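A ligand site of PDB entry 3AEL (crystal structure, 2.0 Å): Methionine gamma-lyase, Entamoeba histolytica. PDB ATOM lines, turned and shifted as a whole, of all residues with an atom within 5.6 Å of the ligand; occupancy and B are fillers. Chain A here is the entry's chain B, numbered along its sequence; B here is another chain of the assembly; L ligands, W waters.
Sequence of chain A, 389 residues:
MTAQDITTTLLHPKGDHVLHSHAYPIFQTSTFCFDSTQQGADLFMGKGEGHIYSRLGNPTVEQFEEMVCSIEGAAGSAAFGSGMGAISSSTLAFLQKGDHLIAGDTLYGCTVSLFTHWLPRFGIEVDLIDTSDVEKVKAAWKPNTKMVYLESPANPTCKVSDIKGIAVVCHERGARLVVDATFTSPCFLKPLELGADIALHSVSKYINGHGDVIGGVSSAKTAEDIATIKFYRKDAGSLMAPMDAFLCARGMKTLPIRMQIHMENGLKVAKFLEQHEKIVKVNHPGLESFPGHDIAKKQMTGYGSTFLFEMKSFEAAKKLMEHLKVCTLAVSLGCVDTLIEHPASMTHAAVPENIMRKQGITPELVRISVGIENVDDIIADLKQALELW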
ATOM      1  N   SER A  82     -21.398  -2.480   8.155  1.00  0.00           N
ATOM      2  CA  SER A  82     -21.852  -2.900   6.814  1.00  0.00           C
ATOM      3  C   SER A  82     -22.227  -1.671   6.013  1.00  0.00           C
ATOM      4  O   SER A  82     -22.470  -0.610   6.594  1.00  0.00           O
ATOM      5  CB  SER A  82     -23.059  -3.865   6.849  1.00  0.00           C
ATOM      6  OG  SER A  82     -24.156  -3.286   7.513  1.00  0.00           O
ATOM      7  N   GLY A  83     -22.271  -1.811   4.690  1.00  0.00           N
ATOM      8  CA  GLY A  83     -22.840  -0.744   3.858  1.00  0.00           C
ATOM      9  C   GLY A  83     -24.272  -0.421   4.301  1.00  0.00           C
ATOM     10  O   GLY A  83     -24.645   0.735   4.306  1.00  0.00           O
ATOM     11  N   MET A  84     -25.055  -1.431   4.707  1.00  0.00           N
ATOM     12  CA  MET A  84     -26.413  -1.135   5.169  1.00  0.00           C
ATOM     13  C   MET A  84     -26.409  -0.285   6.453  1.00  0.00           C
ATOM     14  O   MET A  84     -27.278   0.585   6.603  1.00  0.00           O
ATOM     15  CB  MET A  84     -27.278  -2.400   5.361  1.00  0.00           C
ATOM     16  CG  MET A  84     -27.664  -3.109   4.026  1.00  0.00           C
ATOM     17  SD  MET A  84     -28.193  -2.065   2.659  1.00  0.00           S
ATOM     18  CE  MET A  84     -29.666  -1.258   3.351  1.00  0.00           C
ATOM     19  N   GLY A  85     -25.458  -0.524   7.349  1.00  0.00           N
ATOM     20  CA  GLY A  85     -25.273   0.393   8.528  1.00  0.00           C
ATOM     21  C   GLY A  85     -24.993   1.841   8.077  1.00  0.00           C
ATOM     22  O   GLY A  85     -25.558   2.832   8.620  1.00  0.00           O
ATOM     23  N   ILE A  87     -25.837   3.223   5.194  1.00  0.00           N
ATOM     24  CA  ILE A  87     -27.039   3.738   4.527  1.00  0.00           C
ATOM     25  C   ILE A  87     -28.100   4.142   5.573  1.00  0.00           C
ATOM     26  O   ILE A  87     -28.669   5.246   5.500  1.00  0.00           O
ATOM     27  CB  ILE A  87     -27.603   2.742   3.491  1.00  0.00           C
ATOM     28  CG1 ILE A  87     -26.623   2.660   2.295  1.00  0.00           C
ATOM     29  CG2 ILE A  87     -28.964   3.220   3.002  1.00  0.00           C
ATOM     30  CD1 ILE A  87     -26.844   1.449   1.348  1.00  0.00           C
ATOM     31  N   TYR A 108     -29.789  -1.104  -4.803  1.00  0.00           N
ATOM     32  CA  TYR A 108     -29.478  -2.385  -4.202  1.00  0.00           C
ATOM     33  C   TYR A 108     -30.740  -2.895  -3.461  1.00  0.00           C
ATOM     34  O   TYR A 108     -31.465  -2.121  -2.842  1.00  0.00           O
ATOM     35  CB  TYR A 108     -28.238  -2.253  -3.272  1.00  0.00           C
ATOM     36  CG  TYR A 108     -28.046  -3.476  -2.426  1.00  0.00           C
ATOM     37  CD1 TYR A 108     -27.871  -4.729  -3.018  1.00  0.00           C
ATOM     38  CD2 TYR A 108     -28.106  -3.408  -1.035  1.00  0.00           C
ATOM     39  CE1 TYR A 108     -27.742  -5.876  -2.235  1.00  0.00           C
ATOM     40  CE2 TYR A 108     -27.966  -4.555  -0.260  1.00  0.00           C
ATOM     41  CZ  TYR A 108     -27.780  -5.773  -0.859  1.00  0.00           C
ATOM     42  OH  TYR A 108     -27.653  -6.940  -0.106  1.00  0.00           O
ATOM     43  N   CYS A 110     -31.507  -4.637  -0.621  1.00  0.00           N
ATOM     44  CA  CYS A 110     -31.786  -4.305   0.806  1.00  0.00           C
ATOM     45  C   CYS A 110     -32.011  -2.815   1.037  1.00  0.00           C
ATOM     46  O   CYS A 110     -32.727  -2.434   1.960  1.00  0.00           O
ATOM     47  CB  CYS A 110     -30.702  -4.856   1.726  1.00  0.00           C
ATOM     48  SG  CYS A 110     -30.663  -6.654   1.640  1.00  0.00           S
ATOM     49  N   THR A 111     -31.421  -1.954   0.211  1.00  0.00           N
ATOM     50  CA  THR A 111     -31.732  -0.537   0.274  1.00  0.00           C
ATOM     51  C   THR A 111     -33.203  -0.326  -0.079  1.00  0.00           C
ATOM     52  O   THR A 111     -33.899   0.504   0.525  1.00  0.00           O
ATOM     53  CB  THR A 111     -30.828   0.266  -0.673  1.00  0.00           C
ATOM     54  OG1 THR A 111     -29.454   0.042  -0.337  1.00  0.00           O
ATOM     55  CG2 THR A 111     -31.152   1.754  -0.587  1.00  0.00           C
ATOM     56  N   TYR A 149     -31.872  10.564  -2.345  1.00  0.00           N
ATOM     57  CA  TYR A 149     -30.874   9.496  -2.166  1.00  0.00           C
ATOM     58  C   TYR A 149     -30.666   8.819  -3.531  1.00  0.00           C
ATOM     59  O   TYR A 149     -31.635   8.422  -4.167  1.00  0.00           O
ATOM     60  CB  TYR A 149     -31.327   8.493  -1.097  1.00  0.00           C
ATOM     61  CG  TYR A 149     -30.374   7.329  -0.877  1.00  0.00           C
ATOM     62  CD1 TYR A 149     -30.313   6.268  -1.765  1.00  0.00           C
ATOM     63  CD2 TYR A 149     -29.523   7.300   0.238  1.00  0.00           C
ATOM     64  CE1 TYR A 149     -29.433   5.200  -1.570  1.00  0.00           C
ATOM     65  CE2 TYR A 149     -28.656   6.228   0.450  1.00  0.00           C
ATOM     66  CZ  TYR A 149     -28.599   5.208  -0.478  1.00  0.00           C
ATOM     67  OH  TYR A 149     -27.757   4.146  -0.302  1.00  0.00           O
ATOM     68  N   GLU A 151     -28.048   6.178  -6.147  1.00  0.00           N
ATOM     69  CA  GLU A 151     -26.900   5.317  -6.478  1.00  0.00           C
ATOM     70  C   GLU A 151     -26.625   5.576  -7.946  1.00  0.00           C
ATOM     71  O   GLU A 151     -27.554   5.518  -8.740  1.00  0.00           O
ATOM     72  CB  GLU A 151     -27.264   3.848  -6.417  1.00  0.00           C
ATOM     73  CG  GLU A 151     -27.135   3.129  -5.101  1.00  0.00           C
ATOM     74  CD  GLU A 151     -27.652   1.701  -5.226  1.00  0.00           C
ATOM     75  OE1 GLU A 151     -27.393   1.079  -6.284  1.00  0.00           O
ATOM     76  OE2 GLU A 151     -28.330   1.222  -4.277  1.00  0.00           O
ATOM     77  N   ASN A 155     -27.187  -0.172  -8.950  1.00  0.00           N
ATOM     78  CA  ASN A 155     -27.053  -1.616  -8.847  1.00  0.00           C
ATOM     79  C   ASN A 155     -28.435  -2.197  -9.158  1.00  0.00           C
ATOM     80  O   ASN A 155     -29.382  -1.945  -8.395  1.00  0.00           O
ATOM     81  CB  ASN A 155     -26.632  -1.989  -7.417  1.00  0.00           C
ATOM     82  CG  ASN A 155     -26.427  -3.500  -7.202  1.00  0.00           C
ATOM     83  OD1 ASN A 155     -26.733  -4.336  -8.061  1.00  0.00           O
ATOM     84  ND2 ASN A 155     -25.889  -3.847  -6.052  1.00  0.00           N
ATOM     85  N   ASP A 180     -24.758   6.976  -2.817  1.00  0.00           N
ATOM     86  CA  ASP A 180     -24.098   5.705  -2.621  1.00  0.00           C
ATOM     87  C   ASP A 180     -23.180   5.453  -3.829  1.00  0.00           C
ATOM     88  O   ASP A 180     -23.658   5.186  -4.944  1.00  0.00           O
ATOM     89  CB  ASP A 180     -25.139   4.588  -2.514  1.00  0.00           C
ATOM     90  CG  ASP A 180     -24.512   3.238  -2.246  1.00  0.00           C
ATOM     91  OD1 ASP A 180     -23.294   3.098  -2.475  1.00  0.00           O
ATOM     92  OD2 ASP A 180     -25.230   2.312  -1.815  1.00  0.00           O
ATOM     93  N   THR A 182     -20.768   3.143  -4.005  1.00  0.00           N
ATOM     94  CA  THR A 182     -20.205   1.787  -3.918  1.00  0.00           C
ATOM     95  C   THR A 182     -19.690   1.226  -5.264  1.00  0.00           C
ATOM     96  O   THR A 182     -18.572   0.725  -5.325  1.00  0.00           O
ATOM     97  CB  THR A 182     -21.258   0.781  -3.368  1.00  0.00           C
ATOM     98  OG1 THR A 182     -21.620   1.149  -2.025  1.00  0.00           O
ATOM     99  CG2 THR A 182     -20.701  -0.634  -3.371  1.00  0.00           C
ATOM    100  N   PHE A 183     -20.495   1.324  -6.332  1.00  0.00           N
ATOM    101  CA  PHE A 183     -20.134   0.692  -7.632  1.00  0.00           C
ATOM    102  C   PHE A 183     -18.923   1.263  -8.329  1.00  0.00           C
ATOM    103  O   PHE A 183     -18.368   0.659  -9.266  1.00  0.00           O
ATOM    104  CB  PHE A 183     -21.342   0.727  -8.579  1.00  0.00           C
ATOM    105  CG  PHE A 183     -22.102  -0.547  -8.661  1.00  0.00           C
ATOM    106  CD1 PHE A 183     -22.303  -1.352  -7.523  1.00  0.00           C
ATOM    107  CD2 PHE A 183     -22.664  -0.953  -9.869  1.00  0.00           C
ATOM    108  CE1 PHE A 183     -23.036  -2.540  -7.610  1.00  0.00           C
ATOM    109  CE2 PHE A 183     -23.385  -2.141  -9.965  1.00  0.00           C
ATOM    110  CZ  PHE A 183     -23.563  -2.945  -8.842  1.00  0.00           C
ATOM    111  N   SER A 202     -20.562   0.746   0.544  1.00  0.00           N
ATOM    112  CA  SER A 202     -20.266  -0.578   1.071  1.00  0.00           C
ATOM    113  C   SER A 202     -18.755  -0.800   0.914  1.00  0.00           C
ATOM    114  O   SER A 202     -18.241  -1.060  -0.198  1.00  0.00           O
ATOM    115  CB  SER A 202     -21.033  -1.670   0.321  1.00  0.00           C
ATOM    116  OG  SER A 202     -20.655  -2.952   0.807  1.00  0.00           O
ATOM    117  N   VAL A 203     -18.036  -0.680   2.021  1.00  0.00           N
ATOM    118  CA  VAL A 203     -16.605  -0.951   2.046  1.00  0.00           C
ATOM    119  C   VAL A 203     -16.343  -2.424   1.731  1.00  0.00           C
ATOM    120  O   VAL A 203     -15.258  -2.752   1.267  1.00  0.00           O
ATOM    121  CB  VAL A 203     -16.002  -0.520   3.405  1.00  0.00           C
ATOM    122  CG1 VAL A 203     -14.581  -0.960   3.517  1.00  0.00           C
ATOM    123  CG2 VAL A 203     -16.064   0.999   3.501  1.00  0.00           C
ATOM    124  N   SER A 204     -17.345  -3.270   1.937  1.00  0.00           N
ATOM    125  CA  SER A 204     -17.339  -4.704   1.575  1.00  0.00           C
ATOM    126  C   SER A 204     -16.911  -4.938   0.122  1.00  0.00           C
ATOM    127  O   SER A 204     -16.439  -6.010  -0.210  1.00  0.00           O
ATOM    128  CB  SER A 204     -18.739  -5.313   1.752  1.00  0.00           C
ATOM    129  OG  SER A 204     -19.348  -4.845   2.953  1.00  0.00           O
ATOM    130  N   LYS A 205     -17.085  -3.937  -0.737  1.00  0.00           N
ATOM    131  CA  LYS A 205     -16.814  -4.093  -2.176  1.00  0.00           C
ATOM    132  C   LYS A 205     -15.394  -3.633  -2.536  1.00  0.00           C
ATOM    133  O   LYS A 205     -14.425  -4.162  -1.986  1.00  0.00           O
ATOM    134  CB  LYS A 205     -17.904  -3.433  -3.035  1.00  0.00           C
ATOM    135  CG  LYS A 205     -19.365  -3.731  -2.536  1.00  0.00           C
ATOM    136  CD  LYS A 205     -19.620  -5.213  -2.279  1.00  0.00           C
ATOM    137  CE  LYS A 205     -21.118  -5.492  -2.110  1.00  0.00           C
ATOM    138  NZ  LYS A 205     -21.261  -6.715  -1.202  1.00  0.00           N
ATOM    139  N   ILE A 214     -17.083  -7.343   5.727  1.00  0.00           N
ATOM    140  CA  ILE A 214     -18.266  -6.531   5.473  1.00  0.00           C
ATOM    141  C   ILE A 214     -18.154  -5.252   6.276  1.00  0.00           C
ATOM    142  O   ILE A 214     -17.859  -5.281   7.454  1.00  0.00           O
ATOM    143  CB  ILE A 214     -19.574  -7.346   5.759  1.00  0.00           C
ATOM    144  CG1 ILE A 214     -19.749  -8.402   4.663  1.00  0.00           C
ATOM    145  CG2 ILE A 214     -20.797  -6.405   5.795  1.00  0.00           C
ATOM    146  CD1 ILE A 214     -20.969  -9.241   4.775  1.00  0.00           C
ATOM    147  N   GLY A 215     -18.366  -4.113   5.634  1.00  0.00           N
ATOM    148  CA  GLY A 215     -18.286  -2.851   6.314  1.00  0.00           C
ATOM    149  C   GLY A 215     -18.863  -1.739   5.486  1.00  0.00           C
ATOM    150  O   GLY A 215     -19.091  -1.911   4.293  1.00  0.00           O
ATOM    151  N   GLY A 216     -19.101  -0.605   6.129  1.00  0.00           N
ATOM    152  CA  GLY A 216     -19.717   0.558   5.486  1.00  0.00           C
ATOM    153  C   GLY A 216     -18.928   1.797   5.836  1.00  0.00           C
ATOM    154  O   GLY A 216     -18.225   1.827   6.850  1.00  0.00           O
ATOM    155  N   VAL A 331     -22.992 -13.812  -4.979  1.00  0.00           N
ATOM    156  CA  VAL A 331     -23.416 -12.416  -4.907  1.00  0.00           C
ATOM    157  C   VAL A 331     -22.212 -11.622  -4.416  1.00  0.00           C
ATOM    158  O   VAL A 331     -21.155 -12.226  -4.158  1.00  0.00           O
ATOM    159  CB  VAL A 331     -24.681 -12.225  -4.024  1.00  0.00           C
ATOM    160  CG1 VAL A 331     -25.873 -13.051  -4.601  1.00  0.00           C
ATOM    161  CG2 VAL A 331     -24.421 -12.618  -2.532  1.00  0.00           C
ATOM    162  N   SER A 332     -22.363 -10.303  -4.275  1.00  0.00           N
ATOM    163  CA  SER A 332     -21.286  -9.367  -3.936  1.00  0.00           C
ATOM    164  C   SER A 332     -20.502  -8.940  -5.185  1.00  0.00           C
ATOM    165  O   SER A 332     -20.759  -9.439  -6.279  1.00  0.00           O
ATOM    166  CB  SER A 332     -20.370  -9.899  -2.808  1.00  0.00           C
ATOM    167  OG  SER A 332     -19.594  -8.848  -2.226  1.00  0.00           O
ATOM    168  N   LEU A 333     -19.587  -7.987  -5.022  1.00  0.00           N
ATOM    169  CA  LEU A 333     -18.856  -7.442  -6.152  1.00  0.00           C
ATOM    170  C   LEU A 333     -17.602  -6.727  -5.668  1.00  0.00           C
ATOM    171  O   LEU A 333     -17.399  -6.565  -4.462  1.00  0.00           O
ATOM    172  CB  LEU A 333     -19.746  -6.457  -6.972  1.00  0.00           C
ATOM    173  CG  LEU A 333     -20.242  -5.307  -6.090  1.00  0.00           C
ATOM    174  CD1 LEU A 333     -19.779  -3.977  -6.606  1.00  0.00           C
ATOM    175  CD2 LEU A 333     -21.750  -5.353  -5.859  1.00  0.00           C
ATOM    176  N   GLU A 341     -23.504 -13.322 -10.987  1.00  0.00           N
ATOM    177  CA  GLU A 341     -24.710 -13.348 -10.182  1.00  0.00           C
ATOM    178  C   GLU A 341     -25.961 -13.264 -11.088  1.00  0.00           C
ATOM    179  O   GLU A 341     -25.896 -12.681 -12.179  1.00  0.00           O
ATOM    180  CB  GLU A 341     -24.629 -12.058  -9.360  1.00  0.00           C
ATOM    181  CG  GLU A 341     -25.491 -11.965  -8.230  1.00  0.00           C
ATOM    182  CD  GLU A 341     -26.597 -10.971  -8.408  1.00  0.00           C
ATOM    183  OE1 GLU A 341     -26.406  -9.804  -8.832  1.00  0.00           O
ATOM    184  OE2 GLU A 341     -27.702 -11.372  -8.059  1.00  0.00           O
ATOM    185  N   MET A 346     -31.508 -13.512  -7.068  1.00  0.00           N
ATOM    186  CA  MET A 346     -30.504 -13.382  -6.020  1.00  0.00           C
ATOM    187  C   MET A 346     -30.538 -11.971  -5.411  1.00  0.00           C
ATOM    188  O   MET A 346     -31.407 -11.707  -4.568  1.00  0.00           O
ATOM    189  CB  MET A 346     -29.117 -13.781  -6.547  1.00  0.00           C
ATOM    190  CG  MET A 346     -29.035 -15.223  -7.113  1.00  0.00           C
ATOM    191  SD  MET A 346     -27.438 -15.677  -7.839  1.00  0.00           S
ATOM    192  CE  MET A 346     -27.872 -17.259  -8.583  1.00  0.00           C
ATOM    193  N   THR A 347     -29.677 -11.064  -5.858  1.00  0.00           N
ATOM    194  CA  THR A 347     -29.545  -9.765  -5.163  1.00  0.00           C
ATOM    195  C   THR A 347     -30.839  -8.941  -5.100  1.00  0.00           C
ATOM    196  O   THR A 347     -31.065  -8.185  -4.137  1.00  0.00           O
ATOM    197  CB  THR A 347     -28.428  -8.877  -5.764  1.00  0.00           C
ATOM    198  OG1 THR A 347     -28.609  -8.749  -7.183  1.00  0.00           O
ATOM    199  CG2 THR A 347     -27.029  -9.432  -5.426  1.00  0.00           C
ATOM    200  N   HIS A 348     -31.697  -9.128  -6.101  1.00  0.00           N
ATOM    201  CA  HIS A 348     -32.941  -8.386  -6.210  1.00  0.00           C
ATOM    202  C   HIS A 348     -34.174  -9.285  -6.135  1.00  0.00           C
ATOM    203  O   HIS A 348     -35.284  -8.865  -6.508  1.00  0.00           O
ATOM    204  CB  HIS A 348     -32.919  -7.506  -7.495  1.00  0.00           C
ATOM    205  CG  HIS A 348     -31.925  -6.389  -7.394  1.00  0.00           C
ATOM    206  ND1 HIS A 348     -30.556  -6.616  -7.356  1.00  0.00           N
ATOM    207  CD2 HIS A 348     -32.090  -5.062  -7.209  1.00  0.00           C
ATOM    208  CE1 HIS A 348     -29.928  -5.465  -7.199  1.00  0.00           C
ATOM    209  NE2 HIS A 348     -30.834  -4.503  -7.111  1.00  0.00           N
ATOM    210  N   ARG A 367     -25.360 -10.348 -14.009  1.00  0.00           N
ATOM    211  CA  ARG A 367     -24.458  -9.306 -13.530  1.00  0.00           C
ATOM    212  C   ARG A 367     -23.071  -9.906 -13.289  1.00  0.00           C
ATOM    213  O   ARG A 367     -22.929 -10.913 -12.604  1.00  0.00           O
ATOM    214  CB  ARG A 367     -25.014  -8.584 -12.298  1.00  0.00           C
ATOM    215  CG  ARG A 367     -24.345  -7.267 -11.981  1.00  0.00           C
ATOM    216  CD  ARG A 367     -24.628  -6.773 -10.539  1.00  0.00           C
ATOM    217  NE  ARG A 367     -23.968  -7.609  -9.543  1.00  0.00           N
ATOM    218  CZ  ARG A 367     -24.207  -7.569  -8.217  1.00  0.00           C
ATOM    219  NH1 ARG A 367     -25.068  -6.693  -7.701  1.00  0.00           N
ATOM    220  NH2 ARG A 367     -23.563  -8.392  -7.395  1.00  0.00           N
ATOM    221  N   PHE B  44     -31.897 -18.020  -1.265  1.00  0.00           N
ATOM    222  CA  PHE B  44     -32.526 -16.698  -1.162  1.00  0.00           C
ATOM    223  C   PHE B  44     -34.020 -16.804  -0.774  1.00  0.00           C
ATOM    224  O   PHE B  44     -34.523 -15.927  -0.084  1.00  0.00           O
ATOM    225  CB  PHE B  44     -32.320 -15.866  -2.442  1.00  0.00           C
ATOM    226  CG  PHE B  44     -31.092 -14.972  -2.401  1.00  0.00           C
ATOM    227  CD1 PHE B  44     -29.923 -15.337  -3.033  1.00  0.00           C
ATOM    228  CD2 PHE B  44     -31.126 -13.756  -1.678  1.00  0.00           C
ATOM    229  CE1 PHE B  44     -28.793 -14.521  -2.989  1.00  0.00           C
ATOM    230  CE2 PHE B  44     -30.013 -12.925  -1.633  1.00  0.00           C
ATOM    231  CZ  PHE B  44     -28.837 -13.307  -2.281  1.00  0.00           C
ATOM    232  N   ILE B  52     -24.953 -17.540   2.149  1.00  0.00           N
ATOM    233  CA  ILE B  52     -25.058 -16.640   0.994  1.00  0.00           C
ATOM    234  C   ILE B  52     -24.055 -15.515   1.123  1.00  0.00           C
ATOM    235  O   ILE B  52     -23.282 -15.235   0.189  1.00  0.00           O
ATOM    236  CB  ILE B  52     -26.470 -15.995   0.895  1.00  0.00           C
ATOM    237  CG1 ILE B  52     -27.550 -17.043   0.558  1.00  0.00           C
ATOM    238  CG2 ILE B  52     -26.469 -14.850  -0.164  1.00  0.00           C
ATOM    239  CD1 ILE B  52     -28.990 -16.513   0.738  1.00  0.00           C
ATOM    240  N   TYR B  53     -24.066 -14.861   2.297  1.00  0.00           N
ATOM    241  CA  TYR B  53     -23.397 -13.571   2.473  1.00  0.00           C
ATOM    242  C   TYR B  53     -23.425 -13.264   3.940  1.00  0.00           C
ATOM    243  O   TYR B  53     -24.477 -13.432   4.597  1.00  0.00           O
ATOM    244  CB  TYR B  53     -24.152 -12.482   1.670  1.00  0.00           C
ATOM    245  CG  TYR B  53     -23.466 -11.112   1.650  1.00  0.00           C
ATOM    246  CD1 TYR B  53     -22.310 -10.895   0.872  1.00  0.00           C
ATOM    247  CD2 TYR B  53     -24.019 -10.021   2.342  1.00  0.00           C
ATOM    248  CE1 TYR B  53     -21.674  -9.627   0.834  1.00  0.00           C
ATOM    249  CE2 TYR B  53     -23.404  -8.751   2.311  1.00  0.00           C
ATOM    250  CZ  TYR B  53     -22.237  -8.561   1.537  1.00  0.00           C
ATOM    251  OH  TYR B  53     -21.621  -7.330   1.491  1.00  0.00           O
ATOM    252  N   ARG B  55     -23.597 -10.786   5.980  1.00  0.00           N
ATOM    253  CA  ARG B  55     -24.640  -9.950   6.589  1.00  0.00           C
ATOM    254  C   ARG B  55     -25.934 -10.756   6.872  1.00  0.00           C
ATOM    255  O   ARG B  55     -26.663 -10.461   7.847  1.00  0.00           O
ATOM    256  CB  ARG B  55     -24.971  -8.701   5.741  1.00  0.00           C
ATOM    257  CG  ARG B  55     -26.092  -7.856   6.401  1.00  0.00           C
ATOM    258  CD  ARG B  55     -26.110  -6.347   5.956  1.00  0.00           C
ATOM    259  NE  ARG B  55     -25.853  -6.241   4.514  1.00  0.00           N
ATOM    260  CZ  ARG B  55     -26.687  -6.552   3.527  1.00  0.00           C
ATOM    261  NH1 ARG B  55     -27.918  -6.952   3.791  1.00  0.00           N
ATOM    262  NH2 ARG B  55     -26.268  -6.430   2.261  1.00  0.00           N
ATOM    263  N   LEU B  56     -26.243 -11.714   5.988  1.00  0.00           N
ATOM    264  CA  LEU B  56     -27.418 -12.555   6.154  1.00  0.00           C
ATOM    265  C   LEU B  56     -27.115 -13.707   7.131  1.00  0.00           C
ATOM    266  O   LEU B  56     -27.984 -14.122   7.915  1.00  0.00           O
ATOM    267  CB  LEU B  56     -27.887 -13.098   4.796  1.00  0.00           C
ATOM    268  CG  LEU B  56     -28.109 -12.089   3.665  1.00  0.00           C
ATOM    269  CD1 LEU B  56     -28.667 -12.835   2.439  1.00  0.00           C
ATOM    270  CD2 LEU B  56     -29.101 -11.011   4.049  1.00  0.00           C
HETATM  271  C1  LIG L   1     -24.597  -7.175  -4.099  1.00  0.00           C
HETATM  272  N1  LIG L   1     -24.492  -5.308  -2.562  1.00  0.00           N
HETATM  273  O1  LIG L   1     -24.108  -8.261  -4.433  1.00  0.00           O
HETATM  274  P1  LIG L   1     -23.247  -4.273   2.762  1.00  0.00           P
HETATM  275  N2  LIG L   1     -24.843  -0.335  -1.719  1.00  0.00           N
HETATM  276  C2  LIG L   1     -24.669  -1.031  -2.869  1.00  0.00           C
HETATM  277  C3  LIG L   1     -24.522  -2.405  -2.781  1.00  0.00           C
HETATM  278  O2  LIG L   1     -24.336  -3.100  -3.939  1.00  0.00           O
HETATM  279  C4  LIG L   1     -24.531  -3.090  -1.540  1.00  0.00           C
HETATM  280  C5  LIG L   1     -24.777  -2.349  -0.379  1.00  0.00           C
HETATM  281  C6  LIG L   1     -24.915  -0.955  -0.491  1.00  0.00           C
HETATM  282  C7  LIG L   1     -24.502  -6.666  -2.702  1.00  0.00           C
HETATM  283  C8  LIG L   1     -24.483  -7.616  -1.488  1.00  0.00           C
HETATM  284  S1  LIG L   1     -26.469  -9.660  -1.072  1.00  0.00           S
HETATM  285  C9  LIG L   1     -28.035  -9.538  -1.886  1.00  0.00           C
HETATM  286  C10 LIG L   1     -24.971  -9.043  -1.836  1.00  0.00           C
HETATM  287  C11 LIG L   1     -24.617  -0.330  -4.247  1.00  0.00           C
HETATM  288  C12 LIG L   1     -24.449  -4.588  -1.492  1.00  0.00           C
HETATM  289  C13 LIG L   1     -24.832  -3.014   1.023  1.00  0.00           C
HETATM  290  O3  LIG L   1     -21.786  -4.040   3.027  1.00  0.00           O
HETATM  291  O4  LIG L   1     -23.600  -5.539   2.069  1.00  0.00           O
HETATM  292  O5  LIG L   1     -24.262  -3.953   3.820  1.00  0.00           O
HETATM  293  O6  LIG L   1     -23.521  -3.104   1.602  1.00  0.00           O
HETATM  294  O7  LIG L   1     -25.216  -6.494  -4.968  1.00  0.00           O
HETATM  295  O   HOH W   1     -24.685   1.113  -7.205  1.00  0.00           O
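The side-chain hydroxyl (OG) of Ser 204 sits at hydrogen-bond distance from the backbone NH (N) of Gly 215 (2.9 Å). OH of Tyr 149 lies close to OD2 of Asp 180 (3.5 Å). The side-chain amide oxygen (OD1) of Asn 155 is in hydrogen-bond range of the guanidinium group (NH1) of Arg 367, 2.9 Å away. The side-chain carboxylate (OE1) of Glu 151 lies within hydrogen-bond range of the backbone NH (N) of Asn 155, 3.0 Å away. The side-chain hydroxyl (OH) of Tyr 53 of chain B lies within hydrogen-bond range of the side-chain amino group (NZ) of Lys 205 (2.8 Å). The side-chain carboxylate (OE2) of Glu 151 is in hydrogen-bond range of the backbone NH (N) of Tyr 108 (2.8 Å). The side-chain sulfur (SG) of Cys 110 is in hydrogen-bond range of the side-chain hydroxyl (OH) of Tyr 108, at 3.5 Å. N of Val 203 lies within hydrogen-bond range of O of Gly 215.
Residues that only touch the ligand: Ser 82 (3.3 Å), Ile 87 (3.6 Å), Glu 151 (3.7 Å), Thr 182 (3.6 Å), Phe 183 (3.9 Å), Lys 205 (3.4 Å), Ile 214 (3.8 Å), Gly 215 (3.7 Å), Val 331 (3.7 Å), Leu 333 (3.8 Å), Thr 347 (3.3 Å) and Phe 44 of chain B (3.9 Å). Hydrophobic or aromatic side chains within 4 Å of the ligand: Met 84, Ile 87, Tyr 108, Phe 183, Ile 214, Val 331, Leu 333, Phe 44 of chain B and Tyr 53 of chain B. 23 residues have an atom within 4 Å of the ligand: Ser 82, Gly 83, Met 84, Ile 87, Tyr 108, Glu 151, Asn 155, Asp 180, Thr 182, Phe 183, Ser 202, Ser 204, Lys 205, Ile 214, Gly 215, Val 331, Ser 332, Leu 333, Thr 347, Arg 367, Phe 44 of chain B, Tyr 53 of chain B and Arg 55 of chain B. Along chain A the residues within 4 Å of the ligand span positions 82 to 367. The nearest printed residue that does not touch the ligand is Thr 111 (4.6 Å).
OG of Ser 204 is in hydrogen-bond range of O3 of the ligand (2.6 Å). N2 of the ligand is in hydrogen-bond range of OD2 of Asp 180 (2.7 Å). The backbone NH of Ser 332 is in hydrogen-bond range of an oxygen (O1) of the ligand (2.7 Å). The side-chain hydroxyl of Ser 202 sits at hydrogen-bond distance from an oxygen (O3) of the ligand, 2.7 Å away. O2 of the ligand is in hydrogen-bond range of ND2 of Asn 155 (2.7 Å). An oxygen (O4) of the ligand is in hydrogen-bond range of the side-chain hydroxyl (OH) of Tyr 53 of chain B (2.7 Å). NH1 of Arg 367 is in salt-bridge range of O7 of the ligand (2.7 Å). The backbone NH (N) of Met 84 lies within hydrogen-bond range of an oxygen (O5) of the ligand. An oxygen (O4) of the ligand lies within salt-bridge range of the guanidinium group (NH2) of Arg 55 of chain B (2.8 Å). The backbone NH of Gly 83 lies within hydrogen-bond range of an oxygen (O3) of the ligand, at 2.8 Å. S1 of the ligand sits close to OH of Tyr 108 (3.1 Å).
Water W1 bridges OE1 of Glu 151 and N of Asn 155.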
